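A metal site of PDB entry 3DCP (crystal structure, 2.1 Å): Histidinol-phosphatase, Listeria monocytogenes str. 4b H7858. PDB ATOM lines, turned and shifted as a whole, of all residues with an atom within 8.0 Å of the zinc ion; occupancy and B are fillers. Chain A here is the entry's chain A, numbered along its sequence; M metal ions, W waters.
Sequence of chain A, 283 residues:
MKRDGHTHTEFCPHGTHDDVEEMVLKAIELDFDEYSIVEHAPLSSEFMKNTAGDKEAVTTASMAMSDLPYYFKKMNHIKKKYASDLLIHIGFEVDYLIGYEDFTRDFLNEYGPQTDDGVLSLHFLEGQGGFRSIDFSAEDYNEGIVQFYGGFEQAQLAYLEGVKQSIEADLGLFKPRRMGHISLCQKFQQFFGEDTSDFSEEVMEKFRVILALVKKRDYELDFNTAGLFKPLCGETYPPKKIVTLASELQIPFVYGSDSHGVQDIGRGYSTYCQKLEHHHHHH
A ring nitrogen (ND1) of His 40 lies close to the side-chain carboxylate of Glu 93, 3.5 Å away.
A ring nitrogen (ND1) of His 260 lies within hydrogen-bond range of the backbone carbonyl oxygen (O) of Asp 258 (2.6 Å).
The side-chain sulfur (SG) of Cys 12 is in hydrogen-bond range of the backbone NH (N) of Gly 15 (3.5 Å).
A ring nitrogen (ND1) of His 14 lies within hydrogen-bond range of the backbone carbonyl oxygen (O) of Thr 60.
ND1 of His 14 lies close to SG of Cys 12, at 3.6 Å.
The zinc ion is bound by a ring nitrogen (NE2) of His 260 (2.3 Å), a ring nitrogen (NE2) of His 40 (2.3 Å) and a ring nitrogen (NE2) of His 14 (2.3 Å).
Slightly farther from the zinc ion lies water W1 (2.8 Å).
Residues that only touch the zinc ion: Cys 12 (3.8 Å).
Four residues have an atom within 4 Å of the zinc ion: Cys 12, His 14, His 40 and His 260.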
ATOM      1  N   HIS A   6       7.255  10.416  -5.045  1.00  0.00           N
ATOM      2  CA  HIS A   6       7.632   9.260  -5.841  1.00  0.00           C
ATOM      3  C   HIS A   6       8.406   8.224  -5.035  1.00  0.00           C
ATOM      4  O   HIS A   6       9.627   8.327  -4.890  1.00  0.00           O
ATOM      5  CB  HIS A   6       8.442   9.750  -7.051  1.00  0.00           C
ATOM      6  CG  HIS A   6       8.565   8.753  -8.162  1.00  0.00           C
ATOM      7  ND1 HIS A   6       8.845   9.133  -9.461  1.00  0.00           N
ATOM      8  CD2 HIS A   6       8.472   7.401  -8.173  1.00  0.00           C
ATOM      9  CE1 HIS A   6       8.912   8.049 -10.220  1.00  0.00           C
ATOM     10  NE2 HIS A   6       8.689   6.995  -9.464  1.00  0.00           N
ATOM     11  N   THR A   7       7.694   7.245  -4.491  1.00  0.00           N
ATOM     12  CA  THR A   7       8.344   6.184  -3.709  1.00  0.00           C
ATOM     13  C   THR A   7       7.771   4.816  -4.046  1.00  0.00           C
ATOM     14  O   THR A   7       6.647   4.695  -4.545  1.00  0.00           O
ATOM     15  CB  THR A   7       8.208   6.411  -2.199  1.00  0.00           C
ATOM     16  OG1 THR A   7       6.849   6.171  -1.816  1.00  0.00           O
ATOM     17  CG2 THR A   7       8.616   7.847  -1.836  1.00  0.00           C
ATOM     18  N   HIS A   8       8.535   3.769  -3.754  1.00  0.00           N
ATOM     19  CA  HIS A   8       8.109   2.415  -4.039  1.00  0.00           C
ATOM     20  C   HIS A   8       8.064   1.528  -2.792  1.00  0.00           C
ATOM     21  O   HIS A   8       8.416   1.980  -1.699  1.00  0.00           O
ATOM     22  CB  HIS A   8       9.006   1.833  -5.125  1.00  0.00           C
ATOM     23  CG  HIS A   8       8.803   2.472  -6.455  1.00  0.00           C
ATOM     24  ND1 HIS A   8       7.792   2.105  -7.320  1.00  0.00           N
ATOM     25  CD2 HIS A   8       9.427   3.526  -7.046  1.00  0.00           C
ATOM     26  CE1 HIS A   8       7.811   2.878  -8.384  1.00  0.00           C
ATOM     27  NE2 HIS A   8       8.792   3.756  -8.243  1.00  0.00           N
ATOM     28  N   THR A   9       7.628   0.286  -2.954  1.00  0.00           N
ATOM     29  CA  THR A   9       7.449  -0.614  -1.821  1.00  0.00           C
ATOM     30  C   THR A   9       7.955  -2.030  -2.051  1.00  0.00           C
ATOM     31  O   THR A   9       8.596  -2.323  -3.061  1.00  0.00           O
ATOM     32  CB  THR A   9       5.951  -0.737  -1.472  1.00  0.00           C
ATOM     33  OG1 THR A   9       5.283  -1.499  -2.503  1.00  0.00           O
ATOM     34  CG2 THR A   9       5.302   0.629  -1.377  1.00  0.00           C
ATOM     35  N   CYS A  12       7.351  -4.115  -5.256  1.00  0.00           N
ATOM     36  CA  CYS A  12       8.136  -3.895  -6.467  1.00  0.00           C
ATOM     37  C   CYS A  12       9.122  -5.038  -6.630  1.00  0.00           C
ATOM     38  O   CYS A  12      10.021  -5.216  -5.814  1.00  0.00           O
ATOM     39  CB  CYS A  12       8.893  -2.564  -6.379  1.00  0.00           C
ATOM     40  SG  CYS A  12       9.940  -2.259  -7.817  1.00  0.00           S
ATOM     41  N   PRO A  13       8.974  -5.832  -7.694  1.00  0.00           N
ATOM     42  CA  PRO A  13       9.850  -6.978  -7.951  1.00  0.00           C
ATOM     43  C   PRO A  13      11.343  -6.667  -8.010  1.00  0.00           C
ATOM     44  O   PRO A  13      12.167  -7.487  -7.609  1.00  0.00           O
ATOM     45  CB  PRO A  13       9.319  -7.528  -9.266  1.00  0.00           C
ATOM     46  CG  PRO A  13       7.870  -7.127  -9.259  1.00  0.00           C
ATOM     47  CD  PRO A  13       7.964  -5.704  -8.758  1.00  0.00           C
ATOM     48  N   HIS A  14      11.699  -5.479  -8.494  1.00  0.00           N
ATOM     49  CA  HIS A  14      13.106  -5.121  -8.585  1.00  0.00           C
ATOM     50  C   HIS A  14      13.569  -4.185  -7.479  1.00  0.00           C
ATOM     51  O   HIS A  14      14.670  -3.625  -7.544  1.00  0.00           O
ATOM     52  CB  HIS A  14      13.417  -4.476  -9.935  1.00  0.00           C
ATOM     53  CG  HIS A  14      12.508  -3.335 -10.283  1.00  0.00           C
ATOM     54  ND1 HIS A  14      11.274  -3.531 -10.864  1.00  0.00           N
ATOM     55  CD2 HIS A  14      12.637  -2.001 -10.108  1.00  0.00           C
ATOM     56  CE1 HIS A  14      10.682  -2.361 -11.024  1.00  0.00           C
ATOM     57  NE2 HIS A  14      11.485  -1.415 -10.572  1.00  0.00           N
ATOM     58  N   GLY A  15      12.727  -3.984  -6.473  1.00  0.00           N
ATOM     59  CA  GLY A  15      13.104  -3.130  -5.357  1.00  0.00           C
ATOM     60  C   GLY A  15      14.019  -3.860  -4.394  1.00  0.00           C
ATOM     61  O   GLY A  15      14.416  -5.005  -4.634  1.00  0.00           O
ATOM     62  N   VAL A  38       3.641   5.389  -5.006  1.00  0.00           N
ATOM     63  CA  VAL A  38       3.213   5.204  -6.372  1.00  0.00           C
ATOM     64  C   VAL A  38       3.932   3.992  -6.958  1.00  0.00           C
ATOM     65  O   VAL A  38       4.874   4.111  -7.737  1.00  0.00           O
ATOM     66  CB  VAL A  38       3.506   6.455  -7.203  1.00  0.00           C
ATOM     67  CG1 VAL A  38       2.520   7.561  -6.827  1.00  0.00           C
ATOM     68  CG2 VAL A  38       4.934   6.942  -6.924  1.00  0.00           C
ATOM     69  N   GLU A  39       3.483   2.814  -6.544  1.00  0.00           N
ATOM     70  CA  GLU A  39       4.082   1.587  -6.997  1.00  0.00           C
ATOM     71  C   GLU A  39       3.807   1.359  -8.493  1.00  0.00           C
ATOM     72  O   GLU A  39       2.847   1.880  -9.044  1.00  0.00           O
ATOM     73  CB  GLU A  39       3.552   0.410  -6.190  1.00  0.00           C
ATOM     74  CG  GLU A  39       4.295  -0.853  -6.464  1.00  0.00           C
ATOM     75  CD  GLU A  39       5.787  -0.654  -6.272  1.00  0.00           C
ATOM     76  OE1 GLU A  39       6.238  -0.648  -5.102  1.00  0.00           O
ATOM     77  OE2 GLU A  39       6.486  -0.481  -7.273  1.00  0.00           O
ATOM     78  N   HIS A  40       4.682   0.580  -9.130  1.00  0.00           N
ATOM     79  CA  HIS A  40       4.513   0.276 -10.541  1.00  0.00           C
ATOM     80  C   HIS A  40       3.215  -0.475 -10.838  1.00  0.00           C
ATOM     81  O   HIS A  40       2.941  -1.528 -10.245  1.00  0.00           O
ATOM     82  CB  HIS A  40       5.679  -0.567 -11.038  1.00  0.00           C
ATOM     83  CG  HIS A  40       6.965   0.183 -11.110  1.00  0.00           C
ATOM     84  ND1 HIS A  40       7.227   1.110 -12.101  1.00  0.00           N
ATOM     85  CD2 HIS A  40       8.063   0.161 -10.326  1.00  0.00           C
ATOM     86  CE1 HIS A  40       8.423   1.628 -11.924  1.00  0.00           C
ATOM     87  NE2 HIS A  40       8.958   1.072 -10.842  1.00  0.00           N
ATOM     88  N   THR A  60      10.373  -8.463 -14.184  1.00  0.00           N
ATOM     89  CA  THR A  60      10.669  -7.735 -12.962  1.00  0.00           C
ATOM     90  C   THR A  60      10.069  -6.324 -12.906  1.00  0.00           C
ATOM     91  O   THR A  60      10.062  -5.676 -11.841  1.00  0.00           O
ATOM     92  CB  THR A  60      12.217  -7.710 -12.776  1.00  0.00           C
ATOM     93  OG1 THR A  60      12.634  -8.851 -12.021  1.00  0.00           O
ATOM     94  CG2 THR A  60      12.686  -6.462 -12.095  1.00  0.00           C
ATOM     95  N   ALA A  61       9.523  -5.862 -14.027  1.00  0.00           N
ATOM     96  CA  ALA A  61       8.944  -4.518 -14.138  1.00  0.00           C
ATOM     97  C   ALA A  61       7.967  -4.128 -13.043  1.00  0.00           C
ATOM     98  O   ALA A  61       8.106  -3.064 -12.433  1.00  0.00           O
ATOM     99  CB  ALA A  61       8.292  -4.346 -15.513  1.00  0.00           C
ATOM    100  N   SER A  62       6.963  -4.957 -12.771  1.00  0.00           N
ATOM    101  CA  SER A  62       5.980  -4.622 -11.748  1.00  0.00           C
ATOM    102  C   SER A  62       5.229  -5.825 -11.211  1.00  0.00           C
ATOM    103  O   SER A  62       5.402  -6.950 -11.685  1.00  0.00           O
ATOM    104  CB  SER A  62       4.976  -3.617 -12.293  1.00  0.00           C
ATOM    105  OG  SER A  62       4.148  -4.250 -13.251  1.00  0.00           O
ATOM    106  N   GLU A  93       2.779   4.426 -10.317  1.00  0.00           N
ATOM    107  CA  GLU A  93       3.658   5.032 -11.302  1.00  0.00           C
ATOM    108  C   GLU A  93       3.132   4.276 -12.527  1.00  0.00           C
ATOM    109  O   GLU A  93       3.416   3.095 -12.701  1.00  0.00           O
ATOM    110  CB  GLU A  93       5.120   4.692 -11.098  1.00  0.00           C
ATOM    111  CG  GLU A  93       5.944   5.070 -12.313  1.00  0.00           C
ATOM    112  CD  GLU A  93       7.426   5.116 -12.044  1.00  0.00           C
ATOM    113  OE1 GLU A  93       7.891   4.372 -11.174  1.00  0.00           O
ATOM    114  OE2 GLU A  93       8.126   5.892 -12.728  1.00  0.00           O
ATOM    115  N   HIS A 123       8.907   4.163 -19.882  1.00  0.00           N
ATOM    116  CA  HIS A 123      10.004   3.238 -19.572  1.00  0.00           C
ATOM    117  C   HIS A 123      10.374   2.327 -20.744  1.00  0.00           C
ATOM    118  O   HIS A 123      11.465   1.744 -20.766  1.00  0.00           O
ATOM    119  CB  HIS A 123       9.643   2.332 -18.385  1.00  0.00           C
ATOM    120  CG  HIS A 123       9.477   3.060 -17.090  1.00  0.00           C
ATOM    121  ND1 HIS A 123       8.332   2.950 -16.325  1.00  0.00           N
ATOM    122  CD2 HIS A 123      10.298   3.914 -16.429  1.00  0.00           C
ATOM    123  CE1 HIS A 123       8.465   3.691 -15.240  1.00  0.00           C
ATOM    124  NE2 HIS A 123       9.648   4.292 -15.282  1.00  0.00           N
ATOM    125  N   ASP A 135      15.541   1.958 -19.204  1.00  0.00           N
ATOM    126  CA  ASP A 135      16.347   2.024 -17.985  1.00  0.00           C
ATOM    127  C   ASP A 135      16.886   0.741 -17.324  1.00  0.00           C
ATOM    128  O   ASP A 135      17.384   0.799 -16.200  1.00  0.00           O
ATOM    129  CB  ASP A 135      15.545   2.808 -16.930  1.00  0.00           C
ATOM    130  CG  ASP A 135      14.233   2.133 -16.593  1.00  0.00           C
ATOM    131  OD1 ASP A 135      13.895   1.146 -17.264  1.00  0.00           O
ATOM    132  OD2 ASP A 135      13.534   2.579 -15.657  1.00  0.00           O
ATOM    133  N   HIS A 181      10.148  11.527 -14.286  1.00  0.00           N
ATOM    134  CA  HIS A 181      11.523  11.720 -14.768  1.00  0.00           C
ATOM    135  C   HIS A 181      11.634  11.897 -16.284  1.00  0.00           C
ATOM    136  O   HIS A 181      12.058  10.984 -16.981  1.00  0.00           O
ATOM    137  CB  HIS A 181      12.360  10.505 -14.346  1.00  0.00           C
ATOM    138  CG  HIS A 181      11.678   9.191 -14.584  1.00  0.00           C
ATOM    139  ND1 HIS A 181      11.172   8.816 -15.808  1.00  0.00           N
ATOM    140  CD2 HIS A 181      11.408   8.168 -13.737  1.00  0.00           C
ATOM    141  CE1 HIS A 181      10.625   7.616 -15.719  1.00  0.00           C
ATOM    142  NE2 HIS A 181      10.750   7.200 -14.473  1.00  0.00           N
ATOM    143  N   ASP A 258      12.166   8.580  -5.751  1.00  0.00           N
ATOM    144  CA  ASP A 258      12.079   7.316  -6.471  1.00  0.00           C
ATOM    145  C   ASP A 258      12.688   6.213  -5.590  1.00  0.00           C
ATOM    146  O   ASP A 258      13.355   5.301  -6.094  1.00  0.00           O
ATOM    147  CB  ASP A 258      12.850   7.401  -7.793  1.00  0.00           C
ATOM    148  CG  ASP A 258      12.171   6.601  -8.892  1.00  0.00           C
ATOM    149  OD1 ASP A 258      11.502   5.604  -8.586  1.00  0.00           O
ATOM    150  OD2 ASP A 258      12.323   6.973 -10.077  1.00  0.00           O
ATOM    151  N   SER A 259      12.448   6.290  -4.289  1.00  0.00           N
ATOM    152  CA  SER A 259      12.993   5.323  -3.336  1.00  0.00           C
ATOM    153  C   SER A 259      12.457   3.907  -3.512  1.00  0.00           C
ATOM    154  O   SER A 259      11.242   3.692  -3.657  1.00  0.00           O
ATOM    155  CB  SER A 259      12.730   5.778  -1.893  1.00  0.00           C
ATOM    156  OG  SER A 259      13.411   6.982  -1.580  1.00  0.00           O
ATOM    157  N   HIS A 260      13.358   2.933  -3.503  1.00  0.00           N
ATOM    158  CA  HIS A 260      13.001   1.524  -3.611  1.00  0.00           C
ATOM    159  C   HIS A 260      13.485   0.801  -2.367  1.00  0.00           C
ATOM    160  O   HIS A 260      13.509  -0.428  -2.305  1.00  0.00           O
ATOM    161  CB  HIS A 260      13.638   0.889  -4.851  1.00  0.00           C
ATOM    162  CG  HIS A 260      13.071   1.395  -6.143  1.00  0.00           C
ATOM    163  ND1 HIS A 260      13.249   2.700  -6.561  1.00  0.00           N
ATOM    164  CD2 HIS A 260      12.294   0.804  -7.069  1.00  0.00           C
ATOM    165  CE1 HIS A 260      12.608   2.884  -7.702  1.00  0.00           C
ATOM    166  NE2 HIS A 260      12.018   1.753  -8.034  1.00  0.00           N
HETATM  167 ZN    ZN M   1      11.051   0.774  -9.846  1.00  0.00          ZN
HETATM  168 FE    FE M   2       9.637   5.029  -9.903  1.00  0.00          FE
HETATM  169 FE    FE M   3      10.203   5.209 -13.403  1.00  0.00          FE
HETATM  170  O   HOH W   1      11.855   3.018 -11.364  1.00  0.00           O
